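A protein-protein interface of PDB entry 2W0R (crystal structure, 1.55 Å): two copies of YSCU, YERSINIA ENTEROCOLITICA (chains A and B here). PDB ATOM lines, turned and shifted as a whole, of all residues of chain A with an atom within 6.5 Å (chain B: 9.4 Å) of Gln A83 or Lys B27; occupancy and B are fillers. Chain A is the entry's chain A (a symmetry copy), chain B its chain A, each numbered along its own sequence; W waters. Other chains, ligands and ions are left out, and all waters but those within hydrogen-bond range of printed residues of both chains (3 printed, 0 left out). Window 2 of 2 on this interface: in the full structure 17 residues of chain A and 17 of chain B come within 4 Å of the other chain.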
ATOM      1  N   THR A  55       7.246  -6.398 -11.501  1.00  0.00           N
ATOM      2  CA  THR A  55       7.277  -7.211 -10.286  1.00  0.00           C
ATOM      3  C   THR A  55       6.600  -8.562 -10.417  1.00  0.00           C
ATOM      4  O   THR A  55       6.526  -9.339  -9.447  1.00  0.00           O
ATOM      5  CB  THR A  55       6.770  -6.465  -8.997  1.00  0.00           C
ATOM      6  OG1 THR A  55       5.357  -6.355  -9.001  1.00  0.00           O
ATOM      7  CG2 THR A  55       7.447  -5.090  -8.864  1.00  0.00           C
ATOM      8  N   ASP A  79       8.358 -12.766 -10.716  1.00  0.00           N
ATOM      9  CA  ASP A  79       8.582 -12.182  -9.392  1.00  0.00           C
ATOM     10  C   ASP A  79       9.925 -11.446  -9.325  1.00  0.00           C
ATOM     11  O   ASP A  79      10.198 -10.635 -10.212  1.00  0.00           O
ATOM     12  CB  ASP A  79       8.351 -13.262  -8.297  1.00  0.00           C
ATOM     13  CG  ASP A  79       6.895 -13.584  -8.129  1.00  0.00           C
ATOM     14  OD1 ASP A  79       6.076 -12.674  -8.303  1.00  0.00           O
ATOM     15  OD2 ASP A  79       6.567 -14.738  -7.809  1.00  0.00           O
ATOM     16  N   ALA A  80      10.763 -11.712  -8.321  1.00  0.00           N
ATOM     17  CA  ALA A  80      11.996 -10.928  -8.158  1.00  0.00           C
ATOM     18  C   ALA A  80      12.980 -11.086  -9.300  1.00  0.00           C
ATOM     19  O   ALA A  80      13.835 -10.225  -9.499  1.00  0.00           O
ATOM     20  CB  ALA A  80      12.652 -11.240  -6.792  1.00  0.00           C
ATOM     21  N   GLN A  81      12.846 -12.169 -10.074  1.00  0.00           N
ATOM     22  CA  GLN A  81      13.734 -12.362 -11.242  1.00  0.00           C
ATOM     23  C   GLN A  81      13.549 -11.226 -12.231  1.00  0.00           C
ATOM     24  O   GLN A  81      14.467 -10.921 -13.008  1.00  0.00           O
ATOM     25  CB  GLN A  81      13.460 -13.685 -11.935  1.00  0.00           C
ATOM     26  CG  GLN A  81      13.742 -14.903 -11.116  1.00  0.00           C
ATOM     27  CD  GLN A  81      13.346 -16.158 -11.878  1.00  0.00           C
ATOM     28  OE1 GLN A  81      12.253 -16.241 -12.485  1.00  0.00           O
ATOM     29  NE2 GLN A  81      14.228 -17.138 -11.869  1.00  0.00           N
ATOM     30  N   VAL A  82      12.355 -10.607 -12.245  1.00  0.00           N
ATOM     31  CA  VAL A  82      12.049  -9.494 -13.168  1.00  0.00           C
ATOM     32  C   VAL A  82      12.990  -8.314 -12.918  1.00  0.00           C
ATOM     33  O   VAL A  82      13.442  -7.679 -13.868  1.00  0.00           O
ATOM     34  CB  VAL A  82      10.553  -9.057 -13.085  1.00  0.00           C
ATOM     35  CG1 VAL A  82      10.255  -7.854 -13.999  1.00  0.00           C
ATOM     36  CG2 VAL A  82       9.634 -10.232 -13.433  1.00  0.00           C
ATOM     37  N   GLN A  83      13.302  -8.062 -11.641  1.00  0.00           N
ATOM     38  CA  GLN A  83      14.279  -6.992 -11.255  1.00  0.00           C
ATOM     39  C   GLN A  83      15.644  -7.251 -11.912  1.00  0.00           C
ATOM     40  O   GLN A  83      16.272  -6.334 -12.484  1.00  0.00           O
ATOM     41  CB  GLN A  83      14.406  -6.933  -9.715  1.00  0.00           C
ATOM     42  CG  GLN A  83      13.122  -6.409  -9.030  1.00  0.00           C
ATOM     43  CD  GLN A  83      12.913  -6.902  -7.573  1.00  0.00           C
ATOM     44  OE1 GLN A  83      11.779  -7.229  -7.165  1.00  0.00           O
ATOM     45  NE2 GLN A  83      13.988  -6.975  -6.803  1.00  0.00           N
ATOM     46  N   THR A  84      16.075  -8.502 -11.891  1.00  0.00           N
ATOM     47  CA  THR A  84      17.379  -8.881 -12.428  1.00  0.00           C
ATOM     48  C   THR A  84      17.352  -8.786 -13.958  1.00  0.00           C
ATOM     49  O   THR A  84      18.309  -8.317 -14.586  1.00  0.00           O
ATOM     50  CB  THR A  84      17.814 -10.273 -11.949  1.00  0.00           C
ATOM     51  OG1 THR A  84      17.598 -10.376 -10.518  1.00  0.00           O
ATOM     52  CG2 THR A  84      19.277 -10.537 -12.269  1.00  0.00           C
ATOM     53  N   VAL A  85      16.221  -9.218 -14.548  1.00  0.00           N
ATOM     54  CA  VAL A  85      16.046  -9.093 -15.987  1.00  0.00           C
ATOM     55  C   VAL A  85      16.171  -7.639 -16.422  1.00  0.00           C
ATOM     56  O   VAL A  85      16.843  -7.354 -17.423  1.00  0.00           O
ATOM     57  CB  VAL A  85      14.684  -9.723 -16.468  1.00  0.00           C
ATOM     58  CG1 VAL A  85      14.377  -9.313 -17.935  1.00  0.00           C
ATOM     59  CG2 VAL A  85      14.734 -11.208 -16.347  1.00  0.00           C
ATOM     60  N   ARG A  86      15.541  -6.724 -15.675  1.00  0.00           N
ATOM     61  CA  ARG A  86      15.573  -5.286 -16.038  1.00  0.00           C
ATOM     62  C   ARG A  86      16.992  -4.727 -15.926  1.00  0.00           C
ATOM     63  O   ARG A  86      17.417  -3.945 -16.794  1.00  0.00           O
ATOM     64  CB  ARG A  86      14.574  -4.447 -15.227  1.00  0.00           C
ATOM     65  CG  ARG A  86      13.095  -4.850 -15.431  1.00  0.00           C
ATOM     66  CD  ARG A  86      12.074  -3.662 -15.402  1.00  0.00           C
ATOM     67  NE  ARG A  86      12.330  -2.641 -14.376  1.00  0.00           N
ATOM     68  CZ  ARG A  86      11.596  -1.537 -14.177  1.00  0.00           C
ATOM     69  NH1 ARG A  86      11.944  -0.683 -13.221  1.00  0.00           N
ATOM     70  NH2 ARG A  86      10.518  -1.272 -14.924  1.00  0.00           N
ATOM     71  N   LYS A  87      17.725  -5.145 -14.893  1.00  0.00           N
ATOM     72  CA  LYS A  87      19.122  -4.701 -14.725  1.00  0.00           C
ATOM     73  C   LYS A  87      19.993  -5.199 -15.902  1.00  0.00           C
ATOM     74  O   LYS A  87      20.723  -4.405 -16.520  1.00  0.00           O
ATOM     75  CB  LYS A  87      19.680  -5.193 -13.384  1.00  0.00           C
ATOM     76  CG  LYS A  87      21.092  -4.675 -13.089  1.00  0.00           C
ATOM     77  CD  LYS A  87      21.971  -5.674 -12.336  1.00  0.00           C
ATOM     78  CE  LYS A  87      21.661  -5.835 -10.868  1.00  0.00           C
ATOM     79  NZ  LYS A  87      20.527  -6.733 -10.651  1.00  0.00           N
ATOM     80  N   ILE A  88      19.898  -6.498 -16.216  1.00  0.00           N
ATOM     81  CA  ILE A  88      20.651  -7.102 -17.325  1.00  0.00           C
ATOM     82  C   ILE A  88      20.280  -6.454 -18.653  1.00  0.00           C
ATOM     83  O   ILE A  88      21.174  -6.137 -19.457  1.00  0.00           O
ATOM     84  CB  ILE A  88      20.487  -8.647 -17.381  1.00  0.00           C
ATOM     85  CG1 ILE A  88      21.052  -9.270 -16.097  1.00  0.00           C
ATOM     86  CG2 ILE A  88      21.167  -9.255 -18.672  1.00  0.00           C
ATOM     87  CD1 ILE A  88      20.753 -10.773 -15.883  1.00  0.00           C
ATOM     88  N   SER B  21       6.831  -2.815  -0.230  1.00  0.00           N
ATOM     89  CA  SER B  21       6.694  -2.297  -1.588  1.00  0.00           C
ATOM     90  C   SER B  21       6.321  -3.449  -2.558  1.00  0.00           C
ATOM     91  O   SER B  21       6.515  -4.594  -2.197  1.00  0.00           O
ATOM     92  CB  SER B  21       8.031  -1.716  -2.032  1.00  0.00           C
ATOM     93  OG  SER B  21       9.024  -2.760  -2.148  1.00  0.00           O
ATOM     94  N   PRO B  22       5.800  -3.149  -3.791  1.00  0.00           N
ATOM     95  CA  PRO B  22       5.578  -4.285  -4.748  1.00  0.00           C
ATOM     96  C   PRO B  22       6.853  -5.104  -5.017  1.00  0.00           C
ATOM     97  O   PRO B  22       6.792  -6.347  -5.210  1.00  0.00           O
ATOM     98  CB  PRO B  22       5.116  -3.578  -6.033  1.00  0.00           C
ATOM     99  CG  PRO B  22       4.462  -2.328  -5.523  1.00  0.00           C
ATOM    100  CD  PRO B  22       5.341  -1.868  -4.384  1.00  0.00           C
ATOM    101  N   GLU B  23       7.994  -4.427  -5.017  1.00  0.00           N
ATOM    102  CA  GLU B  23       9.286  -5.108  -5.256  1.00  0.00           C
ATOM    103  C   GLU B  23       9.603  -6.080  -4.107  1.00  0.00           C
ATOM    104  O   GLU B  23      10.015  -7.242  -4.363  1.00  0.00           O
ATOM    105  CB  GLU B  23      10.402  -4.093  -5.469  1.00  0.00           C
ATOM    106  CG  GLU B  23      10.299  -3.272  -6.776  1.00  0.00           C
ATOM    107  CD  GLU B  23       9.191  -2.169  -6.799  1.00  0.00           C
ATOM    108  OE1 GLU B  23       8.656  -1.731  -5.724  1.00  0.00           O
ATOM    109  OE2 GLU B  23       8.862  -1.733  -7.932  1.00  0.00           O
ATOM    110  N   ILE B  24       9.452  -5.657  -2.824  1.00  0.00           N
ATOM    111  CA  ILE B  24       9.738  -6.595  -1.744  1.00  0.00           C
ATOM    112  C   ILE B  24       8.709  -7.760  -1.721  1.00  0.00           C
ATOM    113  O   ILE B  24       9.083  -8.907  -1.405  1.00  0.00           O
ATOM    114  CB  ILE B  24       9.948  -5.902  -0.341  1.00  0.00           C
ATOM    115  CG1 ILE B  24      10.642  -6.871   0.628  1.00  0.00           C
ATOM    116  CG2 ILE B  24       8.659  -5.386   0.201  1.00  0.00           C
ATOM    117  CD1 ILE B  24      11.062  -6.276   1.967  1.00  0.00           C
ATOM    118  N   LYS B  25       7.431  -7.472  -2.071  1.00  0.00           N
ATOM    119  CA  LYS B  25       6.424  -8.536  -2.137  1.00  0.00           C
ATOM    120  C   LYS B  25       6.872  -9.614  -3.137  1.00  0.00           C
ATOM    121  O   LYS B  25       6.743 -10.816  -2.843  1.00  0.00           O
ATOM    122  CB  LYS B  25       4.991  -8.020  -2.426  1.00  0.00           C
ATOM    123  CG  LYS B  25       4.520  -6.884  -1.490  1.00  0.00           C
ATOM    124  CD  LYS B  25       3.016  -6.876  -1.185  1.00  0.00           C
ATOM    125  CE  LYS B  25       2.714  -7.586   0.135  1.00  0.00           C
ATOM    126  NZ  LYS B  25       2.973  -9.063   0.078  1.00  0.00           N
ATOM    127  N   SER B  26       7.430  -9.189  -4.270  1.00  0.00           N
ATOM    128  CA  SER B  26       7.955 -10.137  -5.278  1.00  0.00           C
ATOM    129  C   SER B  26       9.130 -10.963  -4.754  1.00  0.00           C
ATOM    130  O   SER B  26       9.232 -12.179  -5.038  1.00  0.00           O
ATOM    131  CB  SER B  26       8.346  -9.405  -6.531  1.00  0.00           C
ATOM    132  OG  SER B  26       7.196  -8.809  -7.070  1.00  0.00           O
ATOM    133  N   LYS B  27      10.003 -10.305  -3.967  1.00  0.00           N
ATOM    134  CA  LYS B  27      11.134 -11.029  -3.342  1.00  0.00           C
ATOM    135  C   LYS B  27      10.625 -12.035  -2.296  1.00  0.00           C
ATOM    136  O   LYS B  27      11.120 -13.176  -2.234  1.00  0.00           O
ATOM    137  CB  LYS B  27      12.126 -10.061  -2.701  1.00  0.00           C
ATOM    138  CG  LYS B  27      12.856  -9.207  -3.739  1.00  0.00           C
ATOM    139  CD  LYS B  27      13.755  -8.111  -3.170  1.00  0.00           C
ATOM    140  CE  LYS B  27      14.973  -8.726  -2.461  1.00  0.00           C
ATOM    141  NZ  LYS B  27      15.941  -7.623  -2.023  1.00  0.00           N
ATOM    142  N   ARG B  28       9.584 -11.627  -1.531  1.00  0.00           N
ATOM    143  CA  ARG B  28       9.003 -12.488  -0.517  1.00  0.00           C
ATOM    144  C   ARG B  28       8.339 -13.709  -1.162  1.00  0.00           C
ATOM    145  O   ARG B  28       8.477 -14.820  -0.687  1.00  0.00           O
ATOM    146  CB  ARG B  28       8.016 -11.713   0.353  1.00  0.00           C
ATOM    147  CG  ARG B  28       8.716 -10.656   1.277  1.00  0.00           C
ATOM    148  CD  ARG B  28       7.663  -9.832   2.049  1.00  0.00           C
ATOM    149  NE  ARG B  28       6.901 -10.682   2.976  1.00  0.00           N
ATOM    150  CZ  ARG B  28       5.657 -10.461   3.400  1.00  0.00           C
ATOM    151  NH1 ARG B  28       4.952  -9.397   2.989  1.00  0.00           N
ATOM    152  NH2 ARG B  28       5.098 -11.334   4.240  1.00  0.00           N
ATOM    153  N   ARG B  29       7.630 -13.475  -2.271  1.00  0.00           N
ATOM    154  CA  ARG B  29       6.985 -14.607  -2.961  1.00  0.00           C
ATOM    155  C   ARG B  29       8.010 -15.623  -3.412  1.00  0.00           C
ATOM    156  O   ARG B  29       7.875 -16.839  -3.130  1.00  0.00           O
ATOM    157  CB  ARG B  29       6.159 -14.145  -4.167  1.00  0.00           C
ATOM    158  CG  ARG B  29       4.852 -13.466  -3.794  1.00  0.00           C
ATOM    159  CD  ARG B  29       3.929 -13.320  -5.033  1.00  0.00           C
ATOM    160  NE  ARG B  29       4.472 -12.359  -5.987  1.00  0.00           N
ATOM    161  CZ  ARG B  29       4.254 -11.050  -5.966  1.00  0.00           C
ATOM    162  NH1 ARG B  29       3.470 -10.494  -5.035  1.00  0.00           N
ATOM    163  NH2 ARG B  29       4.798 -10.318  -6.912  1.00  0.00           N
ATOM    164  N   GLN B  30       9.071 -15.153  -4.095  1.00  0.00           N
ATOM    165  CA  GLN B  30      10.087 -16.081  -4.576  1.00  0.00           C
ATOM    166  C   GLN B  30      10.784 -16.791  -3.405  1.00  0.00           C
ATOM    167  O   GLN B  30      10.965 -18.010  -3.415  1.00  0.00           O
ATOM    168  CB  GLN B  30      11.101 -15.380  -5.487  1.00  0.00           C
ATOM    169  CG  GLN B  30      12.181 -16.358  -6.020  1.00  0.00           C
ATOM    170  CD  GLN B  30      13.248 -15.702  -6.884  1.00  0.00           C
ATOM    171  OE1 GLN B  30      13.291 -14.477  -7.058  1.00  0.00           O
ATOM    172  NE2 GLN B  30      14.117 -16.538  -7.448  1.00  0.00           N
ATOM    173  N   PHE B  31      11.183 -16.013  -2.402  1.00  0.00           N
ATOM    174  CA  PHE B  31      11.865 -16.601  -1.253  1.00  0.00           C
ATOM    175  C   PHE B  31      11.048 -17.699  -0.543  1.00  0.00           C
ATOM    176  O   PHE B  31      11.561 -18.807  -0.282  1.00  0.00           O
ATOM    177  CB  PHE B  31      12.263 -15.514  -0.249  1.00  0.00           C
ATOM    178  CG  PHE B  31      12.872 -16.089   1.006  1.00  0.00           C
ATOM    179  CD1 PHE B  31      14.180 -16.621   0.984  1.00  0.00           C
ATOM    180  CD2 PHE B  31      12.118 -16.156   2.179  1.00  0.00           C
ATOM    181  CE1 PHE B  31      14.711 -17.213   2.162  1.00  0.00           C
ATOM    182  CE2 PHE B  31      12.658 -16.706   3.355  1.00  0.00           C
ATOM    183  CZ  PHE B  31      13.949 -17.232   3.333  1.00  0.00           C
ATOM    184  N   HIS B  32       9.789 -17.396  -0.245  1.00  0.00           N
ATOM    185  CA  HIS B  32       8.936 -18.378   0.437  1.00  0.00           C
ATOM    186  C   HIS B  32       8.654 -19.605  -0.402  1.00  0.00           C
ATOM    187  O   HIS B  32       8.503 -20.722   0.158  1.00  0.00           O
ATOM    188  CB  HIS B  32       7.717 -17.701   1.073  1.00  0.00           C
ATOM    189  CG  HIS B  32       8.104 -16.844   2.226  1.00  0.00           C
ATOM    190  ND1 HIS B  32       8.503 -17.374   3.443  1.00  0.00           N
ATOM    191  CD2 HIS B  32       8.279 -15.511   2.318  1.00  0.00           C
ATOM    192  CE1 HIS B  32       8.828 -16.384   4.252  1.00  0.00           C
ATOM    193  NE2 HIS B  32       8.719 -15.246   3.593  1.00  0.00           N
ATOM    194  N   GLN B  33       8.607 -19.436  -1.737  1.00  0.00           N
ATOM    195  CA  GLN B  33       8.489 -20.563  -2.663  1.00  0.00           C
ATOM    196  C   GLN B  33       9.777 -21.434  -2.532  1.00  0.00           C
ATOM    197  O   GLN B  33       9.732 -22.664  -2.369  1.00  0.00           O
ATOM    198  CB  GLN B  33       8.298 -19.992  -4.089  1.00  0.00           C
ATOM    199  CG  GLN B  33       7.654 -20.869  -5.219  1.00  0.00           C
ATOM    200  CD  GLN B  33       6.181 -21.240  -4.979  1.00  0.00           C
ATOM    201  OE1 GLN B  33       5.218 -20.620  -5.544  1.00  0.00           O
ATOM    202  NE2 GLN B  33       5.990 -22.254  -4.151  1.00  0.00           N
ATOM    203  N   GLU B  34      10.925 -20.779  -2.605  1.00  0.00           N
ATOM    204  CA  GLU B  34      12.214 -21.497  -2.599  1.00  0.00           C
ATOM    205  C   GLU B  34      12.546 -22.211  -1.296  1.00  0.00           C
ATOM    206  O   GLU B  34      13.155 -23.285  -1.315  1.00  0.00           O
ATOM    207  CB  GLU B  34      13.325 -20.521  -2.954  1.00  0.00           C
ATOM    208  CG  GLU B  34      13.330 -20.130  -4.438  1.00  0.00           C
ATOM    209  CD  GLU B  34      13.656 -21.307  -5.336  1.00  0.00           C
ATOM    210  OE1 GLU B  34      14.674 -21.980  -5.094  1.00  0.00           O
ATOM    211  OE2 GLU B  34      12.863 -21.578  -6.272  1.00  0.00           O
ATOM    212  N   ILE B  35      12.143 -21.634  -0.170  1.00  0.00           N
ATOM    213  CA  ILE B  35      12.461 -22.254   1.126  1.00  0.00           C
ATOM    214  C   ILE B  35      11.519 -23.411   1.469  1.00  0.00           C
ATOM    215  O   ILE B  35      11.814 -24.200   2.374  1.00  0.00           O
ATOM    216  CB  ILE B  35      12.522 -21.206   2.270  1.00  0.00           C
ATOM    217  CG1 ILE B  35      13.437 -21.700   3.407  1.00  0.00           C
ATOM    218  CG2 ILE B  35      11.065 -20.741   2.727  1.00  0.00           C
ATOM    219  CD1 ILE B  35      13.649 -20.701   4.507  1.00  0.00           C
ATOM    220  N   TRP B 108      -0.502 -14.870  -8.932  1.00  0.00           N
ATOM    221  CA  TRP B 108       0.331 -13.672  -9.039  1.00  0.00           C
ATOM    222  C   TRP B 108       0.628 -13.017  -7.710  1.00  0.00           C
ATOM    223  O   TRP B 108       1.741 -12.520  -7.536  1.00  0.00           O
ATOM    224  CB  TRP B 108      -0.341 -12.623  -9.952  1.00  0.00           C
ATOM    225  CG  TRP B 108      -0.509 -13.083 -11.367  1.00  0.00           C
ATOM    226  CD1 TRP B 108      -1.673 -13.240 -12.041  1.00  0.00           C
ATOM    227  CD2 TRP B 108       0.531 -13.474 -12.257  1.00  0.00           C
ATOM    228  NE1 TRP B 108      -1.431 -13.699 -13.342  1.00  0.00           N
ATOM    229  CE2 TRP B 108      -0.087 -13.834 -13.494  1.00  0.00           C
ATOM    230  CE3 TRP B 108       1.928 -13.539 -12.139  1.00  0.00           C
ATOM    231  CZ2 TRP B 108       0.650 -14.286 -14.602  1.00  0.00           C
ATOM    232  CZ3 TRP B 108       2.663 -14.009 -13.218  1.00  0.00           C
ATOM    233  CH2 TRP B 108       2.009 -14.386 -14.443  1.00  0.00           C
ATOM    234  N   LEU B 111       1.427 -15.250  -1.250  1.00  0.00           N
ATOM    235  CA  LEU B 111       2.680 -15.842  -0.797  1.00  0.00           C
ATOM    236  C   LEU B 111       2.380 -17.244  -0.288  1.00  0.00           C
ATOM    237  O   LEU B 111       1.460 -17.420   0.517  1.00  0.00           O
ATOM    238  CB  LEU B 111       3.302 -15.040   0.349  1.00  0.00           C
ATOM    239  CG  LEU B 111       4.171 -13.807   0.036  1.00  0.00           C
ATOM    240  CD1 LEU B 111       3.348 -12.718  -0.681  1.00  0.00           C
ATOM    241  CD2 LEU B 111       4.745 -13.269   1.307  1.00  0.00           C
ATOM    242  N   HIS B 114       1.552 -18.440   3.664  1.00  0.00           N
ATOM    243  CA  HIS B 114       1.031 -17.229   4.289  1.00  0.00           C
ATOM    244  C   HIS B 114      -0.471 -17.141   4.076  1.00  0.00           C
ATOM    245  O   HIS B 114      -1.024 -17.773   3.168  1.00  0.00           O
ATOM    246  CB  HIS B 114       1.704 -15.993   3.679  1.00  0.00           C
ATOM    247  CG  HIS B 114       3.145 -15.852   4.081  1.00  0.00           C
ATOM    248  ND1 HIS B 114       4.143 -16.644   3.558  1.00  0.00           N
ATOM    249  CD2 HIS B 114       3.746 -15.027   4.976  1.00  0.00           C
ATOM    250  CE1 HIS B 114       5.303 -16.317   4.123  1.00  0.00           C
ATOM    251  NE2 HIS B 114       5.089 -15.340   4.985  1.00  0.00           N
HETATM  252  O   HOH W   1       4.599  -7.397  -6.499  1.00  0.00           O
HETATM  253  O   HOH W   2       3.709 -12.523  -9.306  1.00  0.00           O
HETATM  254  O   HOH W   3       7.155 -16.815  -6.471  1.00  0.00           O
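Of the printed residues of chain B, Gln A81 touches Gln B30. No residue of chain B comes within 4 Å of Val A82. Of the printed residues of chain B, Gln A83 touches Glu B23 (3.3 Å) and Lys B27 (3.8 Å). Of the printed residues of chain A, Pro B22 touches Thr A55 (3.8 Å). Of the printed residues of chain A, Ser B26 touches Thr A55 (2.5 Å), Asp A79 (3.5 Å) and Ala A80 (3.7 Å). Lys B27 touches just these residues of chain A: Ala A80 (3.7 Å) and Gln A83 (3.8 Å). Of the printed residues of chain A, Gln B30 touches Ala A80 (3.3 Å) and Gln A81 (3.8 Å). Phe B31 touches none of the printed residues of chain A. The nearest printed residue of chain B that does not touch Gln A83 is Ser B26 (4.1 Å). The nearest printed residue of chain B that does not touch Gln A81 is Ser B26 (6.2 Å).
NH2 of Arg B29 sits at hydrogen-bond distance from O of Thr A55. The backbone carbonyl oxygen of Thr A55 is in hydrogen-bond range of the side-chain hydroxyl of Ser B26 (2.5 Å). The side-chain carboxylate of Asp A79 is in salt-bridge range of the guanidinium group of Arg B29 (2.8 Å). O of Glu B23 lies close to OE1 of Gln A83.
Of the 11 printed residues of chain A, 5 touch a printed residue of chain B. Printed residues of chain A that touch a printed residue of chain B: Thr A55, Asp A79, Ala A80, Gln A81 and Gln A83. Of the 18 printed residues of chain B, 6 touch a printed residue of chain A. Printed residues of chain B that touch a printed residue of chain A: Pro B22, Glu B23, Ser B26, Lys B27, Arg B29 and Gln B30. Among the printed residues, 12 pairs touch across the chains.
Water W3 lies within hydrogen-bond range of OD2 of Asp A79 (2.5 Å), O of Arg B29 (3.4 Å) and N of Gln B30 (3.5 Å). Water W2 lies within hydrogen-bond range of OD1 of Asp A79 (2.6 Å), O of Trp B108 (2.6 Å) and NE of Arg B29 (3.4 Å). Water W1 lies within hydrogen-bond range of O of Pro B22 (2.8 Å), OG1 of Thr A55 (2.8 Å), NH2 of Arg B29 (3.0 Å) and OG of Ser B26 (3.0 Å).
The guanidinium group (NE) of Arg B29 sits at hydrogen-bond distance from the backbone carbonyl oxygen (O) of Trp B108 (3.1 Å). OG of Ser B26 is in hydrogen-bond range of O of Pro B22, 3.1 Å away. The side-chain hydroxyl (OG) of Ser B21 lies close to the backbone NH (N) of Glu B23 (3.5 Å). The side-chain hydroxyl of Ser B26 is in hydrogen-bond range of the guanidinium group of Arg B29.
No position is printed for both chains. Of the 12 pairs that touch across the chains among the printed residues, none has its exchanged pair printed and touching as well.
Pro B22 touches Thr A55 (O to CB, 3.8 Å). Thr A55 touches Glu B23. O of Ser B26 touches CB of Asp A79, at 3.5 Å. Ser B26 touches Ala A80 (O to N, 3.7 Å). CG of Lys B27 touches CB of Ala A80, at 3.7 Å. Gln B30 touches Ala A80. N of Gln A81 touches OE1 of Gln B30 (3.8 Å). Gln A83 touches Lys B27.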
